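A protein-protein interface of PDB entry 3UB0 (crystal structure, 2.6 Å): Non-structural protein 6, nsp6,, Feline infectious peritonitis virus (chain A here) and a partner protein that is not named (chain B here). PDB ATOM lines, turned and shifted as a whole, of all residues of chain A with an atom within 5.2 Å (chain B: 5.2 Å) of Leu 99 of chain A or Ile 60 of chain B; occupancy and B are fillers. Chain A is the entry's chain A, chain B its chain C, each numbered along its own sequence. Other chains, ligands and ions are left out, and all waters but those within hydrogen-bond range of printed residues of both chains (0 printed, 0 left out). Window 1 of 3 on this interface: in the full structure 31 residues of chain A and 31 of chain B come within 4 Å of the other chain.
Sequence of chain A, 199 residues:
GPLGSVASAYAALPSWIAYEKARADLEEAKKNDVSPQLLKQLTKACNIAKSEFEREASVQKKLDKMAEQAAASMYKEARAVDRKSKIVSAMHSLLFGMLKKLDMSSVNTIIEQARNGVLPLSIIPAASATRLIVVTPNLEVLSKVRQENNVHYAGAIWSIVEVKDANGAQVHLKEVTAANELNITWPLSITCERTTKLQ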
ATOM      1  N   LEU A  94     -13.158  -8.572 -33.416  1.00  0.00           N
ATOM      2  CA  LEU A  94     -12.926  -7.365 -32.633  1.00  0.00           C
ATOM      3  C   LEU A  94     -12.553  -7.702 -31.192  1.00  0.00           C
ATOM      4  O   LEU A  94     -11.494  -7.286 -30.723  1.00  0.00           O
ATOM      5  CB  LEU A  94     -14.183  -6.480 -32.639  1.00  0.00           C
ATOM      6  CG  LEU A  94     -14.032  -5.000 -33.035  1.00  0.00           C
ATOM      7  CD1 LEU A  94     -15.183  -4.193 -32.504  1.00  0.00           C
ATOM      8  CD2 LEU A  94     -12.746  -4.401 -32.541  1.00  0.00           C
ATOM      9  N   LEU A  95     -13.425  -8.470 -30.507  1.00  0.00           N
ATOM     10  CA  LEU A  95     -13.277  -8.906 -29.120  1.00  0.00           C
ATOM     11  C   LEU A  95     -11.919  -9.549 -28.837  1.00  0.00           C
ATOM     12  O   LEU A  95     -11.192  -9.022 -27.995  1.00  0.00           O
ATOM     13  CB  LEU A  95     -14.427  -9.860 -28.741  1.00  0.00           C
ATOM     14  CG  LEU A  95     -14.722 -10.183 -27.274  1.00  0.00           C
ATOM     15  CD1 LEU A  95     -14.315 -11.552 -26.931  1.00  0.00           C
ATOM     16  CD2 LEU A  95     -14.272  -9.093 -26.288  1.00  0.00           C
ATOM     17  N   PHE A  96     -11.567 -10.651 -29.555  1.00  0.00           N
ATOM     18  CA  PHE A  96     -10.306 -11.362 -29.362  1.00  0.00           C
ATOM     19  C   PHE A  96      -9.082 -10.559 -29.753  1.00  0.00           C
ATOM     20  O   PHE A  96      -8.032 -10.706 -29.124  1.00  0.00           O
ATOM     21  CB  PHE A  96     -10.325 -12.746 -30.013  1.00  0.00           C
ATOM     22  CG  PHE A  96     -11.232 -13.722 -29.296  1.00  0.00           C
ATOM     23  CD1 PHE A  96     -10.862 -14.275 -28.081  1.00  0.00           C
ATOM     24  CD2 PHE A  96     -12.452 -14.091 -29.843  1.00  0.00           C
ATOM     25  CE1 PHE A  96     -11.719 -15.149 -27.406  1.00  0.00           C
ATOM     26  CE2 PHE A  96     -13.299 -14.980 -29.177  1.00  0.00           C
ATOM     27  CZ  PHE A  96     -12.938 -15.489 -27.954  1.00  0.00           C
ATOM     28  N   GLY A  97      -9.237  -9.690 -30.751  1.00  0.00           N
ATOM     29  CA  GLY A  97      -8.191  -8.780 -31.184  1.00  0.00           C
ATOM     30  C   GLY A  97      -7.833  -7.799 -30.089  1.00  0.00           C
ATOM     31  O   GLY A  97      -6.653  -7.595 -29.790  1.00  0.00           O
ATOM     32  N   MET A  98      -8.870  -7.233 -29.447  1.00  0.00           N
ATOM     33  CA  MET A  98      -8.735  -6.274 -28.352  1.00  0.00           C
ATOM     34  C   MET A  98      -8.189  -6.891 -27.085  1.00  0.00           C
ATOM     35  O   MET A  98      -7.408  -6.247 -26.389  1.00  0.00           O
ATOM     36  CB  MET A  98     -10.058  -5.596 -28.076  1.00  0.00           C
ATOM     37  CG  MET A  98     -10.540  -4.785 -29.252  1.00  0.00           C
ATOM     38  SD  MET A  98     -12.222  -3.999 -28.870  1.00  0.00           S
ATOM     39  CE  MET A  98     -11.503  -2.415 -27.905  1.00  0.00           C
ATOM     40  N   LEU A  99      -8.579  -8.133 -26.790  1.00  0.00           N
ATOM     41  CA  LEU A  99      -8.109  -8.886 -25.632  1.00  0.00           C
ATOM     42  C   LEU A  99      -6.615  -9.147 -25.745  1.00  0.00           C
ATOM     43  O   LEU A  99      -5.911  -9.062 -24.737  1.00  0.00           O
ATOM     44  CB  LEU A  99      -8.873 -10.213 -25.463  1.00  0.00           C
ATOM     45  CG  LEU A  99     -10.359 -10.138 -25.061  1.00  0.00           C
ATOM     46  CD1 LEU A  99     -10.991 -11.499 -25.139  1.00  0.00           C
ATOM     47  CD2 LEU A  99     -10.549  -9.517 -23.662  1.00  0.00           C
ATOM     48  N   LYS A 100      -6.123  -9.437 -26.973  1.00  0.00           N
ATOM     49  CA  LYS A 100      -4.700  -9.652 -27.197  1.00  0.00           C
ATOM     50  C   LYS A 100      -3.957  -8.334 -27.032  1.00  0.00           C
ATOM     51  O   LYS A 100      -2.958  -8.297 -26.316  1.00  0.00           O
ATOM     52  CB  LYS A 100      -4.399 -10.290 -28.568  1.00  0.00           C
ATOM     53  CG  LYS A 100      -3.199 -11.215 -28.463  1.00  0.00           C
ATOM     54  CD  LYS A 100      -2.559 -11.593 -29.761  1.00  0.00           C
ATOM     55  CE  LYS A 100      -1.559 -12.685 -29.486  1.00  0.00           C
ATOM     56  NZ  LYS A 100      -1.181 -13.421 -30.733  1.00  0.00           N
ATOM     57  N   LYS A 101      -4.496  -7.252 -27.635  1.00  0.00           N
ATOM     58  CA  LYS A 101      -3.962  -5.891 -27.632  1.00  0.00           C
ATOM     59  C   LYS A 101      -3.853  -5.325 -26.213  1.00  0.00           C
ATOM     60  O   LYS A 101      -2.975  -4.499 -25.975  1.00  0.00           O
ATOM     61  CB  LYS A 101      -4.820  -4.986 -28.532  1.00  0.00           C
ATOM     62  CG  LYS A 101      -4.134  -3.707 -29.004  1.00  0.00           C
ATOM     63  CD  LYS A 101      -5.053  -2.844 -29.870  1.00  0.00           C
ATOM     64  CE  LYS A 101      -4.729  -1.360 -29.829  1.00  0.00           C
ATOM     65  NZ  LYS A 101      -5.431  -0.666 -28.713  1.00  0.00           N
ATOM     66  N   LEU A 102      -4.721  -5.775 -25.272  1.00  0.00           N
ATOM     67  CA  LEU A 102      -4.710  -5.358 -23.864  1.00  0.00           C
ATOM     68  C   LEU A 102      -3.394  -5.737 -23.204  1.00  0.00           C
ATOM     69  O   LEU A 102      -2.866  -4.965 -22.395  1.00  0.00           O
ATOM     70  CB  LEU A 102      -5.868  -5.997 -23.079  1.00  0.00           C
ATOM     71  CG  LEU A 102      -7.193  -5.240 -23.027  1.00  0.00           C
ATOM     72  CD1 LEU A 102      -8.243  -6.089 -22.357  1.00  0.00           C
ATOM     73  CD2 LEU A 102      -7.058  -3.907 -22.278  1.00  0.00           C
ATOM     74  N   ASP A 103      -2.859  -6.921 -23.577  1.00  0.00           N
ATOM     75  CA  ASP A 103      -1.597  -7.492 -23.091  1.00  0.00           C
ATOM     76  C   ASP A 103      -1.472  -7.436 -21.553  1.00  0.00           C
ATOM     77  O   ASP A 103      -0.523  -6.871 -20.999  1.00  0.00           O
ATOM     78  CB  ASP A 103      -0.377  -6.911 -23.851  1.00  0.00           C
ATOM     79  CG  ASP A 103       0.968  -7.522 -23.484  1.00  0.00           C
ATOM     80  OD1 ASP A 103       1.067  -8.773 -23.455  1.00  0.00           O
ATOM     81  OD2 ASP A 103       1.910  -6.748 -23.195  1.00  0.00           O
ATOM     82  N   VAL A 107      -5.683 -11.544 -18.419  1.00  0.00           N
ATOM     83  CA  VAL A 107      -6.457 -11.759 -19.647  1.00  0.00           C
ATOM     84  C   VAL A 107      -5.806 -12.886 -20.450  1.00  0.00           C
ATOM     85  O   VAL A 107      -6.509 -13.784 -20.888  1.00  0.00           O
ATOM     86  CB  VAL A 107      -6.688 -10.460 -20.485  1.00  0.00           C
ATOM     87  CG1 VAL A 107      -7.434 -10.762 -21.797  1.00  0.00           C
ATOM     88  CG2 VAL A 107      -7.456  -9.411 -19.672  1.00  0.00           C
ATOM     89  N   ASN A 108      -4.463 -12.886 -20.590  1.00  0.00           N
ATOM     90  CA  ASN A 108      -3.725 -13.938 -21.298  1.00  0.00           C
ATOM     91  C   ASN A 108      -3.932 -15.320 -20.643  1.00  0.00           C
ATOM     92  O   ASN A 108      -4.146 -16.314 -21.357  1.00  0.00           O
ATOM     93  CB  ASN A 108      -2.251 -13.601 -21.398  1.00  0.00           C
ATOM     94  CG  ASN A 108      -1.911 -12.360 -22.211  1.00  0.00           C
ATOM     95  OD1 ASN A 108      -0.800 -11.797 -22.093  1.00  0.00           O
ATOM     96  ND2 ASN A 108      -2.840 -11.902 -23.057  1.00  0.00           N
ATOM     97  N   ILE A 110      -6.591 -16.368 -18.638  1.00  0.00           N
ATOM     98  CA  ILE A 110      -7.972 -16.795 -18.881  1.00  0.00           C
ATOM     99  C   ILE A 110      -8.190 -17.355 -20.299  1.00  0.00           C
ATOM    100  O   ILE A 110      -8.811 -18.418 -20.441  1.00  0.00           O
ATOM    101  CB  ILE A 110      -9.046 -15.799 -18.345  1.00  0.00           C
ATOM    102  CG1 ILE A 110     -10.354 -16.520 -17.948  1.00  0.00           C
ATOM    103  CG2 ILE A 110      -9.272 -14.561 -19.254  1.00  0.00           C
ATOM    104  CD1 ILE A 110     -11.409 -15.635 -17.205  1.00  0.00           C
ATOM    105  N   ILE A 111      -7.585 -16.702 -21.313  1.00  0.00           N
ATOM    106  CA  ILE A 111      -7.662 -17.119 -22.720  1.00  0.00           C
ATOM    107  C   ILE A 111      -6.854 -18.383 -22.997  1.00  0.00           C
ATOM    108  O   ILE A 111      -7.354 -19.263 -23.696  1.00  0.00           O
ATOM    109  CB  ILE A 111      -7.382 -15.956 -23.714  1.00  0.00           C
ATOM    110  CG1 ILE A 111      -8.347 -14.769 -23.480  1.00  0.00           C
ATOM    111  CG2 ILE A 111      -7.390 -16.413 -25.170  1.00  0.00           C
ATOM    112  CD1 ILE A 111      -9.907 -15.074 -23.510  1.00  0.00           C
ATOM    113  N   THR B  13     -13.883  -3.139 -24.684  1.00  0.00           N
ATOM    114  CA  THR B  13     -13.908  -4.607 -24.783  1.00  0.00           C
ATOM    115  C   THR B  13     -15.237  -5.105 -24.174  1.00  0.00           C
ATOM    116  O   THR B  13     -15.937  -5.920 -24.765  1.00  0.00           O
ATOM    117  CB  THR B  13     -12.703  -5.194 -24.037  1.00  0.00           C
ATOM    118  OG1 THR B  13     -11.502  -4.768 -24.674  1.00  0.00           O
ATOM    119  CG2 THR B  13     -12.740  -6.681 -23.978  1.00  0.00           C
ATOM    120  N   LEU B  17     -18.325  -7.413 -25.632  1.00  0.00           N
ATOM    121  CA  LEU B  17     -18.748  -8.604 -24.874  1.00  0.00           C
ATOM    122  C   LEU B  17     -20.254  -8.601 -24.650  1.00  0.00           C
ATOM    123  O   LEU B  17     -20.904  -9.597 -24.947  1.00  0.00           O
ATOM    124  CB  LEU B  17     -18.037  -8.696 -23.511  1.00  0.00           C
ATOM    125  CG  LEU B  17     -16.684  -9.351 -23.473  1.00  0.00           C
ATOM    126  CD1 LEU B  17     -15.979  -8.991 -22.211  1.00  0.00           C
ATOM    127  CD2 LEU B  17     -16.785 -10.851 -23.625  1.00  0.00           C
ATOM    128  N   LEU B  56     -14.295  -7.348 -15.608  1.00  0.00           N
ATOM    129  CA  LEU B  56     -14.090  -7.747 -17.007  1.00  0.00           C
ATOM    130  C   LEU B  56     -13.778  -9.229 -17.058  1.00  0.00           C
ATOM    131  O   LEU B  56     -14.303  -9.935 -17.927  1.00  0.00           O
ATOM    132  CB  LEU B  56     -12.964  -6.929 -17.661  1.00  0.00           C
ATOM    133  CG  LEU B  56     -12.754  -7.095 -19.167  1.00  0.00           C
ATOM    134  CD1 LEU B  56     -13.963  -6.578 -19.962  1.00  0.00           C
ATOM    135  CD2 LEU B  56     -11.475  -6.440 -19.590  1.00  0.00           C
ATOM    136  N   LEU B  57     -12.960  -9.698 -16.094  1.00  0.00           N
ATOM    137  CA  LEU B  57     -12.579 -11.106 -15.948  1.00  0.00           C
ATOM    138  C   LEU B  57     -13.791 -11.977 -15.645  1.00  0.00           C
ATOM    139  O   LEU B  57     -13.881 -13.093 -16.147  1.00  0.00           O
ATOM    140  CB  LEU B  57     -11.509 -11.246 -14.881  1.00  0.00           C
ATOM    141  CG  LEU B  57     -10.051 -10.929 -15.351  1.00  0.00           C
ATOM    142  CD1 LEU B  57      -9.132 -10.816 -14.166  1.00  0.00           C
ATOM    143  CD2 LEU B  57      -9.509 -11.942 -16.355  1.00  0.00           C
ATOM    144  N   ALA B  58     -14.758 -11.433 -14.900  1.00  0.00           N
ATOM    145  CA  ALA B  58     -16.027 -12.093 -14.590  1.00  0.00           C
ATOM    146  C   ALA B  58     -16.919 -12.188 -15.853  1.00  0.00           C
ATOM    147  O   ALA B  58     -17.516 -13.237 -16.090  1.00  0.00           O
ATOM    148  CB  ALA B  58     -16.756 -11.350 -13.469  1.00  0.00           C
ATOM    149  N   LEU B  59     -16.957 -11.116 -16.678  1.00  0.00           N
ATOM    150  CA  LEU B  59     -17.738 -11.078 -17.916  1.00  0.00           C
ATOM    151  C   LEU B  59     -17.163 -12.023 -18.961  1.00  0.00           C
ATOM    152  O   LEU B  59     -17.927 -12.755 -19.590  1.00  0.00           O
ATOM    153  CB  LEU B  59     -17.858  -9.645 -18.448  1.00  0.00           C
ATOM    154  CG  LEU B  59     -19.047  -9.312 -19.393  1.00  0.00           C
ATOM    155  CD1 LEU B  59     -20.421  -9.586 -18.784  1.00  0.00           C
ATOM    156  CD2 LEU B  59     -18.994  -7.890 -19.806  1.00  0.00           C
ATOM    157  N   ILE B  60     -15.831 -12.009 -19.155  1.00  0.00           N
ATOM    158  CA  ILE B  60     -15.118 -12.926 -20.080  1.00  0.00           C
ATOM    159  C   ILE B  60     -15.414 -14.375 -19.701  1.00  0.00           C
ATOM    160  O   ILE B  60     -15.747 -15.169 -20.576  1.00  0.00           O
ATOM    161  CB  ILE B  60     -13.585 -12.648 -20.150  1.00  0.00           C
ATOM    162  CG1 ILE B  60     -13.303 -11.332 -20.887  1.00  0.00           C
ATOM    163  CG2 ILE B  60     -12.847 -13.769 -20.846  1.00  0.00           C
ATOM    164  CD1 ILE B  60     -11.959 -10.638 -20.509  1.00  0.00           C
ATOM    165  N   ALA B  61     -15.296 -14.710 -18.400  1.00  0.00           N
ATOM    166  CA  ALA B  61     -15.587 -16.046 -17.882  1.00  0.00           C
ATOM    167  C   ALA B  61     -17.033 -16.444 -18.223  1.00  0.00           C
ATOM    168  O   ALA B  61     -17.221 -17.519 -18.784  1.00  0.00           O
ATOM    169  CB  ALA B  61     -15.351 -16.097 -16.374  1.00  0.00           C
ATOM    170  N   PHE B  62     -18.036 -15.579 -17.940  1.00  0.00           N
ATOM    171  CA  PHE B  62     -19.452 -15.844 -18.266  1.00  0.00           C
ATOM    172  C   PHE B  62     -19.624 -16.155 -19.779  1.00  0.00           C
ATOM    173  O   PHE B  62     -20.268 -17.138 -20.144  1.00  0.00           O
ATOM    174  CB  PHE B  62     -20.407 -14.703 -17.805  1.00  0.00           C
ATOM    175  CG  PHE B  62     -21.853 -15.136 -17.980  1.00  0.00           C
ATOM    176  CD1 PHE B  62     -22.501 -14.982 -19.200  1.00  0.00           C
ATOM    177  CD2 PHE B  62     -22.533 -15.799 -16.959  1.00  0.00           C
ATOM    178  CE1 PHE B  62     -23.811 -15.453 -19.388  1.00  0.00           C
ATOM    179  CE2 PHE B  62     -23.858 -16.241 -17.142  1.00  0.00           C
ATOM    180  CZ  PHE B  62     -24.482 -16.064 -18.356  1.00  0.00           C
ATOM    181  N   PHE B  63     -18.991 -15.329 -20.629  1.00  0.00           N
ATOM    182  CA  PHE B  63     -18.947 -15.438 -22.090  1.00  0.00           C
ATOM    183  C   PHE B  63     -18.358 -16.775 -22.494  1.00  0.00           C
ATOM    184  O   PHE B  63     -18.923 -17.447 -23.340  1.00  0.00           O
ATOM    185  CB  PHE B  63     -18.121 -14.265 -22.691  1.00  0.00           C
ATOM    186  CG  PHE B  63     -17.802 -14.403 -24.157  1.00  0.00           C
ATOM    187  CD1 PHE B  63     -18.784 -14.198 -25.124  1.00  0.00           C
ATOM    188  CD2 PHE B  63     -16.526 -14.774 -24.577  1.00  0.00           C
ATOM    189  CE1 PHE B  63     -18.497 -14.365 -26.480  1.00  0.00           C
ATOM    190  CE2 PHE B  63     -16.248 -14.970 -25.938  1.00  0.00           C
ATOM    191  CZ  PHE B  63     -17.233 -14.764 -26.878  1.00  0.00           C
ATOM    192  N   LEU B  64     -17.235 -17.156 -21.883  1.00  0.00           N
ATOM    193  CA  LEU B  64     -16.507 -18.415 -22.100  1.00  0.00           C
ATOM    194  C   LEU B  64     -17.396 -19.625 -21.793  1.00  0.00           C
ATOM    195  O   LEU B  64     -17.370 -20.618 -22.516  1.00  0.00           O
ATOM    196  CB  LEU B  64     -15.244 -18.436 -21.201  1.00  0.00           C
ATOM    197  CG  LEU B  64     -13.868 -18.021 -21.773  1.00  0.00           C
ATOM    198  CD1 LEU B  64     -13.945 -17.048 -22.909  1.00  0.00           C
ATOM    199  CD2 LEU B  64     -12.921 -17.553 -20.688  1.00  0.00           C
ATOM    200  N   SER B  65     -18.212 -19.521 -20.744  1.00  0.00           N
ATOM    201  CA  SER B  65     -19.105 -20.600 -20.327  1.00  0.00           C
ATOM    202  C   SER B  65     -20.232 -20.909 -21.328  1.00  0.00           C
ATOM    203  O   SER B  65     -20.725 -22.028 -21.363  1.00  0.00           O
ATOM    204  CB  SER B  65     -19.658 -20.314 -18.934  1.00  0.00           C
ATOM    205  OG  SER B  65     -20.727 -19.378 -18.922  1.00  0.00           O
ATOM    206  N   PHE B  80      -7.598 -14.635 -31.691  1.00  0.00           N
ATOM    207  CA  PHE B  80      -6.711 -14.192 -30.611  1.00  0.00           C
ATOM    208  C   PHE B  80      -5.267 -14.533 -30.983  1.00  0.00           C
ATOM    209  O   PHE B  80      -4.446 -13.631 -31.087  1.00  0.00           O
ATOM    210  CB  PHE B  80      -7.123 -14.841 -29.277  1.00  0.00           C
ATOM    211  CG  PHE B  80      -6.269 -14.460 -28.098  1.00  0.00           C
ATOM    212  CD1 PHE B  80      -6.672 -13.450 -27.224  1.00  0.00           C
ATOM    213  CD2 PHE B  80      -5.050 -15.104 -27.859  1.00  0.00           C
ATOM    214  CE1 PHE B  80      -5.873 -13.089 -26.125  1.00  0.00           C
ATOM    215  CE2 PHE B  80      -4.237 -14.732 -26.775  1.00  0.00           C
ATOM    216  CZ  PHE B  80      -4.645 -13.720 -25.918  1.00  0.00           C
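O of Phe 80 of chain B sits close to NZ of Lys 100 of chain A.
Leu 95 of chain A touches Leu 17 of chain B. CE2 of Phe 63 of chain B touches CZ of Phe 96 of chain A, at 3.9 Å. O of Phe 96 of chain A touches CD1 of Phe 80 of chain B, 3.6 Å away. Thr 13 of chain B touches Met 98 of chain A. Leu 99 of chain A touches Thr 13 of chain B (CD2 to CG2, 3.6 Å). CD1 of Ile 60 of chain B touches CD2 of Leu 99 of chain A, at 3.6 Å. Phe 80 of chain B touches Asn 108 of chain A (CZ to ND2, 3.8 Å). CD1 of Ile 110 of chain A touches O of Leu 57 of chain B, 3.7 Å away. CG2 of Ile 110 of chain A touches CG2 of Ile 60 of chain B, at 3.99 Å. Phe 80 of chain B touches Ile 111 of chain A.
Leu 99 of chain A touches two residues of chain B. Of the printed residues of chain B, Lys 100 of chain A touches Phe 80 (3.1 Å). Printed residues of chain B within 4 Å of Asn 108 of chain A: Phe 80. Printed residues of chain A within 4 Å of Leu 17 of chain B: Leu 95. Ala 58 of chain B touches none of the printed residues of chain A. Printed residues of chain A within 4 Å of Ile 60 of chain B: Leu 99 and Ile 110. Ala 61 of chain B touches none of the printed residues of chain A. Printed residues of chain A within 4 Å of Leu 64 of chain B: Ile 110. The nearest residue of chain B that does not touch Leu 99 of chain A is Phe 80 of chain B (4.03 Å). The nearest printed residue of chain A that does not touch Ile 60 of chain B is Ile 111 of chain A (4.2 Å).
Of the 14 printed residues of chain A, 8 touch a printed residue of chain B. Hydrophobic or aromatic side chains of chain B that line the printed part of chain A: Leu 17, Leu 57, Ile 60, Phe 63, Leu 64 and Phe 80.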
